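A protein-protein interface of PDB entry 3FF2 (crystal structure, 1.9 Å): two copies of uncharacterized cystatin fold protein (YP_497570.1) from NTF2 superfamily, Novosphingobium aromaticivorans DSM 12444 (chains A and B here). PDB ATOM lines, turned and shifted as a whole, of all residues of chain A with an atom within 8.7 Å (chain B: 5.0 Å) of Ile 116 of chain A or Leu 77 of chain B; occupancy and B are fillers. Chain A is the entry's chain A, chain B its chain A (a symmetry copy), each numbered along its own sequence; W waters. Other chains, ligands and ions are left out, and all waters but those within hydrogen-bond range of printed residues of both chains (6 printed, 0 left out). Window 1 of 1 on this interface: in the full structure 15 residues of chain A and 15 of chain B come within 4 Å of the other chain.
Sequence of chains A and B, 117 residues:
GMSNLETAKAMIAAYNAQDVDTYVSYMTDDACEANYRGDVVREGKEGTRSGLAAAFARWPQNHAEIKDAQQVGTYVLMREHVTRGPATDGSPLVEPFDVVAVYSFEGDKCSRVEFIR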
ATOM      1  N   ALA A  34     -33.388   6.520  -0.453  1.00  0.00           N
ATOM      2  CA  ALA A  34     -32.435   6.978  -1.444  1.00  0.00           C
ATOM      3  C   ALA A  34     -31.036   6.414  -1.191  1.00  0.00           C
ATOM      4  O   ALA A  34     -30.674   5.975  -0.078  1.00  0.00           O
ATOM      5  CB  ALA A  34     -32.417   8.547  -1.449  1.00  0.00           C
ATOM      6  N   ASN A  35     -30.251   6.407  -2.252  1.00  0.00           N
ATOM      7  CA  ASN A  35     -28.810   6.163  -2.108  1.00  0.00           C
ATOM      8  C   ASN A  35     -28.133   7.449  -1.644  1.00  0.00           C
ATOM      9  O   ASN A  35     -28.513   8.556  -2.019  1.00  0.00           O
ATOM     10  CB  ASN A  35     -28.210   5.664  -3.395  1.00  0.00           C
ATOM     11  CG  ASN A  35     -28.765   4.335  -3.794  1.00  0.00           C
ATOM     12  OD1 ASN A  35     -28.977   3.427  -2.947  1.00  0.00           O
ATOM     13  ND2 ASN A  35     -29.013   4.189  -5.086  1.00  0.00           N
ATOM     14  N   TYR A  36     -27.222   7.253  -0.708  1.00  0.00           N
ATOM     15  CA  TYR A  36     -26.441   8.322  -0.114  1.00  0.00           C
ATOM     16  C   TYR A  36     -25.785   9.092  -1.238  1.00  0.00           C
ATOM     17  O   TYR A  36     -25.189   8.513  -2.117  1.00  0.00           O
ATOM     18  CB  TYR A  36     -25.386   7.738   0.855  1.00  0.00           C
ATOM     19  CG  TYR A  36     -24.354   8.738   1.336  1.00  0.00           C
ATOM     20  CD1 TYR A  36     -24.705   9.718   2.251  1.00  0.00           C
ATOM     21  CD2 TYR A  36     -23.033   8.691   0.906  1.00  0.00           C
ATOM     22  CE1 TYR A  36     -23.796  10.615   2.701  1.00  0.00           C
ATOM     23  CE2 TYR A  36     -22.110   9.642   1.342  1.00  0.00           C
ATOM     24  CZ  TYR A  36     -22.524  10.604   2.249  1.00  0.00           C
ATOM     25  OH  TYR A  36     -21.675  11.580   2.752  1.00  0.00           O
ATOM     26  N   ARG A  37     -25.939  10.409  -1.181  1.00  0.00           N
ATOM     27  CA  ARG A  37     -25.492  11.335  -2.222  1.00  0.00           C
ATOM     28  C   ARG A  37     -25.909  10.866  -3.606  1.00  0.00           C
ATOM     29  O   ARG A  37     -25.233  11.122  -4.580  1.00  0.00           O
ATOM     30  CB  ARG A  37     -23.978  11.531  -2.177  1.00  0.00           C
ATOM     31  CG  ARG A  37     -23.465  11.968  -0.856  1.00  0.00           C
ATOM     32  CD  ARG A  37     -23.353  13.411  -0.716  1.00  0.00           C
ATOM     33  NE  ARG A  37     -22.634  14.061  -1.795  1.00  0.00           N
ATOM     34  CZ  ARG A  37     -22.915  15.293  -2.213  1.00  0.00           C
ATOM     35  NH1 ARG A  37     -23.907  15.982  -1.670  1.00  0.00           N
ATOM     36  NH2 ARG A  37     -22.252  15.822  -3.207  1.00  0.00           N
ATOM     37  N   ASP A  68     -25.063  -2.720  14.167  1.00  0.00           N
ATOM     38  CA  ASP A  68     -24.681  -1.555  14.994  1.00  0.00           C
ATOM     39  C   ASP A  68     -25.816  -0.585  14.814  1.00  0.00           C
ATOM     40  O   ASP A  68     -26.301  -0.420  13.699  1.00  0.00           O
ATOM     41  CB  ASP A  68     -23.360  -0.943  14.486  1.00  0.00           C
ATOM     42  CG  ASP A  68     -22.797   0.185  15.397  1.00  0.00           C
ATOM     43  OD1 ASP A  68     -22.242  -0.133  16.449  1.00  0.00           O
ATOM     44  OD2 ASP A  68     -22.843   1.383  15.022  1.00  0.00           O
ATOM     45  N   LEU A  77     -28.263   5.834  12.677  1.00  0.00           N
ATOM     46  CA  LEU A  77     -27.465   5.024  11.750  1.00  0.00           C
ATOM     47  C   LEU A  77     -27.462   3.573  12.186  1.00  0.00           C
ATOM     48  O   LEU A  77     -27.240   3.258  13.336  1.00  0.00           O
ATOM     49  CB  LEU A  77     -26.007   5.498  11.628  1.00  0.00           C
ATOM     50  CG  LEU A  77     -25.765   6.906  11.092  1.00  0.00           C
ATOM     51  CD1 LEU A  77     -26.078   7.913  12.215  1.00  0.00           C
ATOM     52  CD2 LEU A  77     -24.304   6.998  10.606  1.00  0.00           C
ATOM     53  N   MET A  78     -27.763   2.706  11.225  1.00  0.00           N
ATOM     54  CA  MET A  78     -27.746   1.295  11.475  1.00  0.00           C
ATOM     55  C   MET A  78     -26.986   0.568  10.420  1.00  0.00           C
ATOM     56  O   MET A  78     -27.290   0.675   9.255  1.00  0.00           O
ATOM     57  CB  MET A  78     -29.190   0.780  11.558  1.00  0.00           C
ATOM     58  CG  MET A  78     -29.844   1.266  12.882  1.00  0.00           C
ATOM     59  SD  MET A  78     -31.441   0.305  13.302  1.00  0.00           S
ATOM     60  CE  MET A  78     -31.982  -0.145  11.667  1.00  0.00           C
ATOM     61  N   ARG A  79     -25.962  -0.141  10.862  1.00  0.00           N
ATOM     62  CA  ARG A  79     -25.204  -1.006   9.987  1.00  0.00           C
ATOM     63  C   ARG A  79     -25.965  -2.330   9.924  1.00  0.00           C
ATOM     64  O   ARG A  79     -26.364  -2.900  10.960  1.00  0.00           O
ATOM     65  CB  ARG A  79     -23.769  -1.164  10.496  1.00  0.00           C
ATOM     66  CG  ARG A  79     -22.846  -1.785   9.521  1.00  0.00           C
ATOM     67  CD  ARG A  79     -21.436  -1.380   9.868  1.00  0.00           C
ATOM     68  NE  ARG A  79     -21.083  -1.676  11.261  1.00  0.00           N
ATOM     69  CZ  ARG A  79     -20.756  -2.889  11.673  1.00  0.00           C
ATOM     70  NH1 ARG A  79     -20.794  -3.899  10.806  1.00  0.00           N
ATOM     71  NH2 ARG A  79     -20.417  -3.103  12.934  1.00  0.00           N
ATOM     72  N   GLU A  80     -26.281  -2.728   8.703  1.00  0.00           N
ATOM     73  CA  GLU A  80     -27.229  -3.839   8.438  1.00  0.00           C
ATOM     74  C   GLU A  80     -26.549  -4.867   7.507  1.00  0.00           C
ATOM     75  O   GLU A  80     -25.822  -4.513   6.571  1.00  0.00           O
ATOM     76  CB  GLU A  80     -28.528  -3.309   7.802  1.00  0.00           C
ATOM     77  CG  GLU A  80     -29.264  -2.276   8.676  1.00  0.00           C
ATOM     78  CD  GLU A  80     -30.488  -1.671   8.034  1.00  0.00           C
ATOM     79  OE1 GLU A  80     -30.848  -2.115   6.941  1.00  0.00           O
ATOM     80  OE2 GLU A  80     -31.072  -0.725   8.635  1.00  0.00           O
ATOM     81  N   PHE A  97     -25.108  -8.812   1.582  1.00  0.00           N
ATOM     82  CA  PHE A  97     -24.320  -7.585   1.503  1.00  0.00           C
ATOM     83  C   PHE A  97     -24.506  -6.740   2.738  1.00  0.00           C
ATOM     84  O   PHE A  97     -25.421  -6.921   3.507  1.00  0.00           O
ATOM     85  CB  PHE A  97     -24.676  -6.756   0.255  1.00  0.00           C
ATOM     86  CG  PHE A  97     -26.103  -6.272   0.197  1.00  0.00           C
ATOM     87  CD1 PHE A  97     -26.476  -5.044   0.739  1.00  0.00           C
ATOM     88  CD2 PHE A  97     -27.088  -7.046  -0.440  1.00  0.00           C
ATOM     89  CE1 PHE A  97     -27.785  -4.615   0.661  1.00  0.00           C
ATOM     90  CE2 PHE A  97     -28.415  -6.593  -0.534  1.00  0.00           C
ATOM     91  CZ  PHE A  97     -28.756  -5.394   0.027  1.00  0.00           C
ATOM     92  N   ASP A  98     -23.622  -5.783   2.888  1.00  0.00           N
ATOM     93  CA  ASP A  98     -23.691  -4.855   4.007  1.00  0.00           C
ATOM     94  C   ASP A  98     -23.997  -3.458   3.544  1.00  0.00           C
ATOM     95  O   ASP A  98     -23.584  -3.036   2.487  1.00  0.00           O
ATOM     96  CB  ASP A  98     -22.399  -4.887   4.800  1.00  0.00           C
ATOM     97  CG  ASP A  98     -22.081  -6.280   5.298  1.00  0.00           C
ATOM     98  OD1 ASP A  98     -22.948  -6.886   5.946  1.00  0.00           O
ATOM     99  OD2 ASP A  98     -20.982  -6.782   5.020  1.00  0.00           O
ATOM    100  N   VAL A  99     -24.784  -2.761   4.347  1.00  0.00           N
ATOM    101  CA  VAL A  99     -25.081  -1.352   4.117  1.00  0.00           C
ATOM    102  C   VAL A  99     -25.089  -0.643   5.458  1.00  0.00           C
ATOM    103  O   VAL A  99     -25.156  -1.268   6.519  1.00  0.00           O
ATOM    104  CB  VAL A  99     -26.452  -1.130   3.446  1.00  0.00           C
ATOM    105  CG1 VAL A  99     -26.475  -1.746   2.085  1.00  0.00           C
ATOM    106  CG2 VAL A  99     -27.586  -1.682   4.316  1.00  0.00           C
ATOM    107  N   VAL A 100     -24.978   0.674   5.388  1.00  0.00           N
ATOM    108  CA  VAL A 100     -25.397   1.544   6.505  1.00  0.00           C
ATOM    109  C   VAL A 100     -26.607   2.355   6.017  1.00  0.00           C
ATOM    110  O   VAL A 100     -26.578   3.066   4.995  1.00  0.00           O
ATOM    111  CB  VAL A 100     -24.265   2.456   7.057  1.00  0.00           C
ATOM    112  CG1 VAL A 100     -24.793   3.415   8.151  1.00  0.00           C
ATOM    113  CG2 VAL A 100     -23.053   1.619   7.510  1.00  0.00           C
ATOM    114  N   ALA A 101     -27.673   2.205   6.791  1.00  0.00           N
ATOM    115  CA  ALA A 101     -28.917   2.949   6.671  1.00  0.00           C
ATOM    116  C   ALA A 101     -28.888   4.139   7.612  1.00  0.00           C
ATOM    117  O   ALA A 101     -28.737   4.000   8.824  1.00  0.00           O
ATOM    118  CB  ALA A 101     -30.137   2.030   6.977  1.00  0.00           C
ATOM    119  N   VAL A 102     -29.009   5.314   7.018  1.00  0.00           N
ATOM    120  CA  VAL A 102     -29.082   6.562   7.751  1.00  0.00           C
ATOM    121  C   VAL A 102     -30.521   7.066   7.710  1.00  0.00           C
ATOM    122  O   VAL A 102     -31.008   7.369   6.651  1.00  0.00           O
ATOM    123  CB  VAL A 102     -28.113   7.610   7.196  1.00  0.00           C
ATOM    124  CG1 VAL A 102     -28.082   8.862   8.141  1.00  0.00           C
ATOM    125  CG2 VAL A 102     -26.691   7.029   7.003  1.00  0.00           C
ATOM    126  N   TYR A 103     -31.158   7.156   8.903  1.00  0.00           N
ATOM    127  CA  TYR A 103     -32.533   7.608   9.079  1.00  0.00           C
ATOM    128  C   TYR A 103     -32.511   9.043   9.486  1.00  0.00           C
ATOM    129  O   TYR A 103     -31.956   9.384  10.514  1.00  0.00           O
ATOM    130  CB  TYR A 103     -33.287   6.806  10.161  1.00  0.00           C
ATOM    131  CG  TYR A 103     -33.343   5.329   9.833  1.00  0.00           C
ATOM    132  CD1 TYR A 103     -32.208   4.541   9.918  1.00  0.00           C
ATOM    133  CD2 TYR A 103     -34.526   4.740   9.402  1.00  0.00           C
ATOM    134  CE1 TYR A 103     -32.238   3.181   9.590  1.00  0.00           C
ATOM    135  CE2 TYR A 103     -34.577   3.375   9.064  1.00  0.00           C
ATOM    136  CZ  TYR A 103     -33.413   2.604   9.162  1.00  0.00           C
ATOM    137  OH  TYR A 103     -33.395   1.254   8.852  1.00  0.00           O
ATOM    138  N   VAL A 113     -34.587   7.854   4.539  1.00  0.00           N
ATOM    139  CA  VAL A 113     -33.681   6.734   4.781  1.00  0.00           C
ATOM    140  C   VAL A 113     -32.722   6.707   3.603  1.00  0.00           C
ATOM    141  O   VAL A 113     -33.137   6.669   2.429  1.00  0.00           O
ATOM    142  CB  VAL A 113     -34.377   5.394   4.899  1.00  0.00           C
ATOM    143  CG1 VAL A 113     -33.379   4.275   5.242  1.00  0.00           C
ATOM    144  CG2 VAL A 113     -35.504   5.456   5.867  1.00  0.00           C
ATOM    145  N   GLU A 114     -31.438   6.755   3.935  1.00  0.00           N
ATOM    146  CA  GLU A 114     -30.408   6.671   2.913  1.00  0.00           C
ATOM    147  C   GLU A 114     -29.498   5.515   3.119  1.00  0.00           C
ATOM    148  O   GLU A 114     -29.209   5.101   4.257  1.00  0.00           O
ATOM    149  CB  GLU A 114     -29.617   7.968   2.799  1.00  0.00           C
ATOM    150  CG  GLU A 114     -30.441   9.130   2.343  1.00  0.00           C
ATOM    151  CD  GLU A 114     -29.559  10.262   1.794  1.00  0.00           C
ATOM    152  OE1 GLU A 114     -28.446  10.479   2.327  1.00  0.00           O
ATOM    153  OE2 GLU A 114     -29.991  10.923   0.844  1.00  0.00           O
ATOM    154  N   PHE A 115     -29.029   4.989   1.990  1.00  0.00           N
ATOM    155  CA  PHE A 115     -28.204   3.799   2.010  1.00  0.00           C
ATOM    156  C   PHE A 115     -26.806   4.074   1.533  1.00  0.00           C
ATOM    157  O   PHE A 115     -26.609   4.622   0.451  1.00  0.00           O
ATOM    158  CB  PHE A 115     -28.862   2.667   1.189  1.00  0.00           C
ATOM    159  CG  PHE A 115     -30.304   2.388   1.592  1.00  0.00           C
ATOM    160  CD1 PHE A 115     -30.597   1.791   2.809  1.00  0.00           C
ATOM    161  CD2 PHE A 115     -31.354   2.776   0.784  1.00  0.00           C
ATOM    162  CE1 PHE A 115     -31.931   1.600   3.187  1.00  0.00           C
ATOM    163  CE2 PHE A 115     -32.653   2.555   1.154  1.00  0.00           C
ATOM    164  CZ  PHE A 115     -32.939   1.970   2.348  1.00  0.00           C
ATOM    165  N   ILE A 116     -25.875   3.675   2.394  1.00  0.00           N
ATOM    166  CA  ILE A 116     -24.429   3.633   2.132  1.00  0.00           C
ATOM    167  C   ILE A 116     -23.985   2.184   1.977  1.00  0.00           C
ATOM    168  O   ILE A 116     -24.118   1.375   2.885  1.00  0.00           O
ATOM    169  CB  ILE A 116     -23.605   4.298   3.278  1.00  0.00           C
ATOM    170  CG1 ILE A 116     -24.114   5.704   3.590  1.00  0.00           C
ATOM    171  CG2 ILE A 116     -22.123   4.351   2.899  1.00  0.00           C
ATOM    172  CD1 ILE A 116     -23.619   6.303   4.895  1.00  0.00           C
ATOM    173  N   ARG A 117     -23.513   1.876   0.773  1.00  0.00           N
ATOM    174  CA  ARG A 117     -23.123   0.529   0.360  1.00  0.00           C
ATOM    175  C   ARG A 117     -21.915   0.613  -0.542  1.00  0.00           C
ATOM    176  O   ARG A 117     -21.095  -0.310  -0.606  1.00  0.00           O
ATOM    177  CB  ARG A 117     -24.253  -0.179  -0.408  1.00  0.00           C
ATOM    178  CG  ARG A 117     -23.828  -1.549  -0.908  1.00  0.00           C
ATOM    179  CD  ARG A 117     -25.006  -2.418  -1.316  1.00  0.00           C
ATOM    180  NE  ARG A 117     -24.534  -3.660  -1.909  1.00  0.00           N
ATOM    181  CZ  ARG A 117     -25.313  -4.475  -2.606  1.00  0.00           C
ATOM    182  NH1 ARG A 117     -26.584  -4.156  -2.774  1.00  0.00           N
ATOM    183  NH2 ARG A 117     -24.830  -5.595  -3.128  1.00  0.00           N
ATOM    184  OXT ARG A 117     -21.720   1.630  -1.226  1.00  0.00           O
ATOM    185  N   ASP B  68     -15.627   4.391  16.492  1.00  0.00           N
ATOM    186  CA  ASP B  68     -16.029   3.270  15.616  1.00  0.00           C
ATOM    187  C   ASP B  68     -15.551   3.678  14.250  1.00  0.00           C
ATOM    188  O   ASP B  68     -15.699   4.838  13.877  1.00  0.00           O
ATOM    189  CB  ASP B  68     -17.562   3.102  15.626  1.00  0.00           C
ATOM    190  CG  ASP B  68     -18.062   1.843  14.862  1.00  0.00           C
ATOM    191  OD1 ASP B  68     -17.941   0.742  15.400  1.00  0.00           O
ATOM    192  OD2 ASP B  68     -18.646   1.965  13.756  1.00  0.00           O
ATOM    193  N   ALA B  69     -14.944   2.745  13.533  1.00  0.00           N
ATOM    194  CA  ALA B  69     -14.463   3.014  12.168  1.00  0.00           C
ATOM    195  C   ALA B  69     -14.807   1.832  11.323  1.00  0.00           C
ATOM    196  O   ALA B  69     -14.416   0.740  11.639  1.00  0.00           O
ATOM    197  CB  ALA B  69     -12.952   3.262  12.135  1.00  0.00           C
ATOM    198  N   GLN B  70     -15.553   2.076  10.262  1.00  0.00           N
ATOM    199  CA  GLN B  70     -16.038   1.028   9.347  1.00  0.00           C
ATOM    200  C   GLN B  70     -15.792   1.430   7.907  1.00  0.00           C
ATOM    201  O   GLN B  70     -15.979   2.581   7.553  1.00  0.00           O
ATOM    202  CB  GLN B  70     -17.545   0.814   9.515  1.00  0.00           C
ATOM    203  CG  GLN B  70     -17.986   0.486  10.932  1.00  0.00           C
ATOM    204  CD  GLN B  70     -17.611  -0.910  11.371  1.00  0.00           C
ATOM    205  OE1 GLN B  70     -17.360  -1.781  10.543  1.00  0.00           O
ATOM    206  NE2 GLN B  70     -17.598  -1.139  12.685  1.00  0.00           N
ATOM    207  N   VAL B  72     -17.424   0.668   4.343  1.00  0.00           N
ATOM    208  CA  VAL B  72     -18.609   0.100   3.698  1.00  0.00           C
ATOM    209  C   VAL B  72     -18.520   0.418   2.188  1.00  0.00           C
ATOM    210  O   VAL B  72     -18.692   1.544   1.767  1.00  0.00           O
ATOM    211  CB  VAL B  72     -19.939   0.625   4.326  1.00  0.00           C
ATOM    212  CG1 VAL B  72     -21.191  -0.017   3.651  1.00  0.00           C
ATOM    213  CG2 VAL B  72     -19.952   0.331   5.836  1.00  0.00           C
ATOM    214  N   TYR B  75     -16.852   3.686   0.904  1.00  0.00           N
ATOM    215  CA  TYR B  75     -17.108   4.723   1.919  1.00  0.00           C
ATOM    216  C   TYR B  75     -16.457   4.298   3.218  1.00  0.00           C
ATOM    217  O   TYR B  75     -16.407   3.112   3.557  1.00  0.00           O
ATOM    218  CB  TYR B  75     -18.587   4.950   2.143  1.00  0.00           C
ATOM    219  CG  TYR B  75     -19.357   5.408   0.924  1.00  0.00           C
ATOM    220  CD1 TYR B  75     -19.426   6.754   0.607  1.00  0.00           C
ATOM    221  CD2 TYR B  75     -20.033   4.496   0.106  1.00  0.00           C
ATOM    222  CE1 TYR B  75     -20.121   7.180  -0.485  1.00  0.00           C
ATOM    223  CE2 TYR B  75     -20.740   4.924  -1.003  1.00  0.00           C
ATOM    224  CZ  TYR B  75     -20.771   6.255  -1.292  1.00  0.00           C
ATOM    225  OH  TYR B  75     -21.475   6.706  -2.362  1.00  0.00           O
ATOM    226  N   VAL B  76     -16.012   5.282   3.982  1.00  0.00           N
ATOM    227  CA  VAL B  76     -15.575   5.068   5.363  1.00  0.00           C
ATOM    228  C   VAL B  76     -16.438   5.919   6.304  1.00  0.00           C
ATOM    229  O   VAL B  76     -16.695   7.097   6.034  1.00  0.00           O
ATOM    230  CB  VAL B  76     -14.075   5.409   5.529  1.00  0.00           C
ATOM    231  CG1 VAL B  76     -13.629   5.290   6.974  1.00  0.00           C
ATOM    232  CG2 VAL B  76     -13.208   4.496   4.626  1.00  0.00           C
ATOM    233  N   LEU B  77     -16.935   5.288   7.376  1.00  0.00           N
ATOM    234  CA  LEU B  77     -17.676   5.977   8.438  1.00  0.00           C
ATOM    235  C   LEU B  77     -16.933   5.868   9.755  1.00  0.00           C
ATOM    236  O   LEU B  77     -16.499   4.806  10.149  1.00  0.00           O
ATOM    237  CB  LEU B  77     -19.101   5.436   8.637  1.00  0.00           C
ATOM    238  CG  LEU B  77     -20.070   5.551   7.463  1.00  0.00           C
ATOM    239  CD1 LEU B  77     -19.717   4.460   6.434  1.00  0.00           C
ATOM    240  CD2 LEU B  77     -21.507   5.412   8.003  1.00  0.00           C
ATOM    241  N   MET B  78     -16.769   7.019  10.395  1.00  0.00           N
ATOM    242  CA  MET B  78     -16.134   7.063  11.679  1.00  0.00           C
ATOM    243  C   MET B  78     -16.930   7.867  12.649  1.00  0.00           C
ATOM    244  O   MET B  78     -17.224   9.013  12.406  1.00  0.00           O
ATOM    245  CB  MET B  78     -14.720   7.644  11.523  1.00  0.00           C
ATOM    246  CG  MET B  78     -13.803   6.604  10.820  1.00  0.00           C
ATOM    247  SD  MET B  78     -11.949   7.026  11.005  1.00  0.00           S
ATOM    248  CE  MET B  78     -12.037   8.797  11.157  1.00  0.00           C
ATOM    249  N   ARG B  79     -17.305   7.213  13.735  1.00  0.00           N
ATOM    250  CA  ARG B  79     -17.968   7.881  14.830  1.00  0.00           C
ATOM    251  C   ARG B  79     -16.866   8.489  15.697  1.00  0.00           C
ATOM    252  O   ARG B  79     -15.876   7.819  16.053  1.00  0.00           O
ATOM    253  CB  ARG B  79     -18.861   6.902  15.598  1.00  0.00           C
ATOM    254  CG  ARG B  79     -19.797   7.550  16.544  1.00  0.00           C
ATOM    255  CD  ARG B  79     -20.955   6.617  16.789  1.00  0.00           C
ATOM    256  NE  ARG B  79     -20.530   5.282  17.226  1.00  0.00           N
ATOM    257  CZ  ARG B  79     -20.154   5.022  18.467  1.00  0.00           C
ATOM    258  NH1 ARG B  79     -20.109   6.016  19.351  1.00  0.00           N
ATOM    259  NH2 ARG B  79     -19.806   3.796  18.822  1.00  0.00           N
ATOM    260  N   VAL B 100     -20.777  11.616  13.354  1.00  0.00           N
ATOM    261  CA  VAL B 100     -20.289  10.598  12.402  1.00  0.00           C
ATOM    262  C   VAL B 100     -19.821  11.344  11.143  1.00  0.00           C
ATOM    263  O   VAL B 100     -20.557  12.117  10.501  1.00  0.00           O
ATOM    264  CB  VAL B 100     -21.325   9.487  12.073  1.00  0.00           C
ATOM    265  CG1 VAL B 100     -20.791   8.515  10.995  1.00  0.00           C
ATOM    266  CG2 VAL B 100     -21.799   8.777  13.356  1.00  0.00           C
ATOM    267  N   ALA B 101     -18.559  11.085  10.830  1.00  0.00           N
ATOM    268  CA  ALA B 101     -17.880  11.525   9.621  1.00  0.00           C
ATOM    269  C   ALA B 101     -17.954  10.431   8.572  1.00  0.00           C
ATOM    270  O   ALA B 101     -17.503   9.307   8.777  1.00  0.00           O
ATOM    271  CB  ALA B 101     -16.399  11.896   9.929  1.00  0.00           C
ATOM    272  N   VAL B 102     -18.563  10.784   7.451  1.00  0.00           N
ATOM    273  CA  VAL B 102     -18.666   9.906   6.304  1.00  0.00           C
ATOM    274  C   VAL B 102     -17.701  10.397   5.228  1.00  0.00           C
ATOM    275  O   VAL B 102     -17.876  11.480   4.732  1.00  0.00           O
ATOM    276  CB  VAL B 102     -20.099   9.829   5.767  1.00  0.00           C
ATOM    277  CG1 VAL B 102     -20.198   8.720   4.663  1.00  0.00           C
ATOM    278  CG2 VAL B 102     -21.121   9.572   6.901  1.00  0.00           C
ATOM    279  N   TYR B 103     -16.702   9.546   4.888  1.00  0.00           N
ATOM    280  CA  TYR B 103     -15.676   9.826   3.890  1.00  0.00           C
ATOM    281  C   TYR B 103     -16.070   9.170   2.609  1.00  0.00           C
ATOM    282  O   TYR B 103     -16.212   7.961   2.554  1.00  0.00           O
ATOM    283  CB  TYR B 103     -14.286   9.296   4.303  1.00  0.00           C
ATOM    284  CG  TYR B 103     -13.816   9.903   5.607  1.00  0.00           C
ATOM    285  CD1 TYR B 103     -14.404   9.545   6.808  1.00  0.00           C
ATOM    286  CD2 TYR B 103     -12.809  10.861   5.625  1.00  0.00           C
ATOM    287  CE1 TYR B 103     -13.999  10.119   8.019  1.00  0.00           C
ATOM    288  CE2 TYR B 103     -12.389  11.452   6.830  1.00  0.00           C
ATOM    289  CZ  TYR B 103     -13.001  11.069   8.029  1.00  0.00           C
ATOM    290  OH  TYR B 103     -12.632  11.606   9.250  1.00  0.00           O
HETATM  291  O   HOH W   1     -19.624  -1.140  14.933  1.00  0.00           O
HETATM  292  O   HOH W   2     -20.914   3.383  15.271  1.00  0.00           O
HETATM  293  O   HOH W   3     -24.288   6.051  -2.596  1.00  0.00           O
HETATM  294  O   HOH W   4     -20.347   1.303  17.418  1.00  0.00           O
HETATM  295  O   HOH W   5     -19.078  11.825   2.221  1.00  0.00           O
HETATM  296  O   HOH W   6     -20.883   0.607  12.784  1.00  0.00           O
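Leu 77 of chain A touches Val 100 of chain B, and with the chains exchanged Val 100 of chain A touches Leu 77 of chain B.
Positions printed for both chains: 68, 77, 78, 79, 100, 101, 102 and 103.
Of the printed residues of chain B, Arg 79 of chain A touches Gln 70 (3.4 Å).
Glu 114 of chain A touches none of the printed residues of chain B.
Ile 116 of chain A touches just these residues of chain B: Val 72 (3.3 Å), Tyr 75 (3.5 Å) and Leu 77 (3.9 Å).
Of the printed residues of chain A, Val 72 of chain B touches Val 100, Ile 116 and Arg 117.
Printed residues of chain A within 4 Å of Tyr 75 of chain B: Tyr 36 (3.6 Å), Ile 116 (3.5 Å) and Arg 117 (3.4 Å).
Leu 77 of chain B touches just these residues of chain A: Val 100 (3.8 Å) and Ile 116 (3.9 Å).
Of the printed residues of chain A, Val 100 of chain B touches Leu 77.
The nearest residue of chain B that does not touch Ile 116 of chain A is Val 102 of chain B (4.2 Å).
The nearest residue of chain A that does not touch Leu 77 of chain B is Leu 77 of chain A (4.1 Å).
Among the printed residues, pairs that only touch across the chains: Tyr 36 of chain A with Tyr 75 of chain B (3.6 Å), Tyr 36 of chain A with Val 102 of chain B (3.7 Å), Leu 77 of chain A with Val 100 of chain B (3.8 Å), Val 100 of chain A with Val 72 of chain B (3.8 Å), Val 100 of chain A with Leu 77 of chain B (3.8 Å), Ile 116 of chain A with Val 72 of chain B (3.3 Å), Ile 116 of chain A with Tyr 75 of chain B (3.5 Å), Ile 116 of chain A with Leu 77 of chain B (3.9 Å), Arg 117 of chain A with Val 72 of chain B (3.9 Å) and Arg 117 of chain A with Tyr 75 of chain B (3.4 Å).
Of the 21 printed residues of chain A, 6 touch a printed residue of chain B.
Hydrophobic or aromatic side chains of chain A that line the printed part of chain B: Tyr 36, Leu 77, Val 100 and Ile 116.
Hydrophobic or aromatic side chains of chain B within 4 Å of the printed part of chain A: Val 72, Tyr 75, Leu 77, Val 100 and Val 102.
The backbone carbonyl oxygen of Phe 115 of chain A lies within hydrogen-bond range of the backbone NH of Tyr 36 of chain A, at 2.9 Å.
OD1 of Asp 68 of chain B lies within hydrogen-bond range of NE2 of Gln 70 of chain B, 3.3 Å away.
The backbone carbonyl oxygen (O) of Gln 70 of chain B lies within hydrogen-bond range of the backbone NH (N) of Leu 77 of chain B.
O of Ile 116 of chain A sits at hydrogen-bond distance from N of Val 100 of chain A.
The backbone NH (N) of Arg 79 of chain A lies within hydrogen-bond range of the backbone carbonyl oxygen (O) of Asp 68 of chain A (2.9 Å).
The side-chain amide nitrogen of Gln 70 of chain B sits close to the guanidinium group of Arg 79 of chain A, at 3.4 Å.
Water W1 lies within hydrogen-bond range of the side-chain carboxylate (OD1) of Asp 68 of chain B (2.6 Å), the guanidinium group (NH2) of Arg 79 of chain A (2.9 Å), the side-chain amide nitrogen (NE2) of Gln 70 of chain B (3.0 Å) and the side-chain carboxylate (OD1) of Asp 68 of chain A (3.2 Å).
Water W4 lies within hydrogen-bond range of OD1 of Asp 68 of chain A, NH2 of Arg 79 of chain B and OD1 of Asp 68 of chain B.
Water W5 lies within hydrogen-bond range of the side-chain hydroxyl of Tyr 36 of chain A and the backbone carbonyl oxygen of Val 102 of chain B.
Water W3 bridges O of Tyr 36 of chain A and OH of Tyr 75 of chain B.
Water W6 lies within hydrogen-bond range of NE of Arg 79 of chain A (2.8 Å), OD2 of Asp 68 of chain B (2.8 Å) and OD2 of Asp 68 of chain A (3.1 Å).
Water W2 lies within hydrogen-bond range of NE of Arg 79 of chain B (2.8 Å), OD2 of Asp 68 of chain A (2.8 Å) and OD2 of Asp 68 of chain B (3.1 Å).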
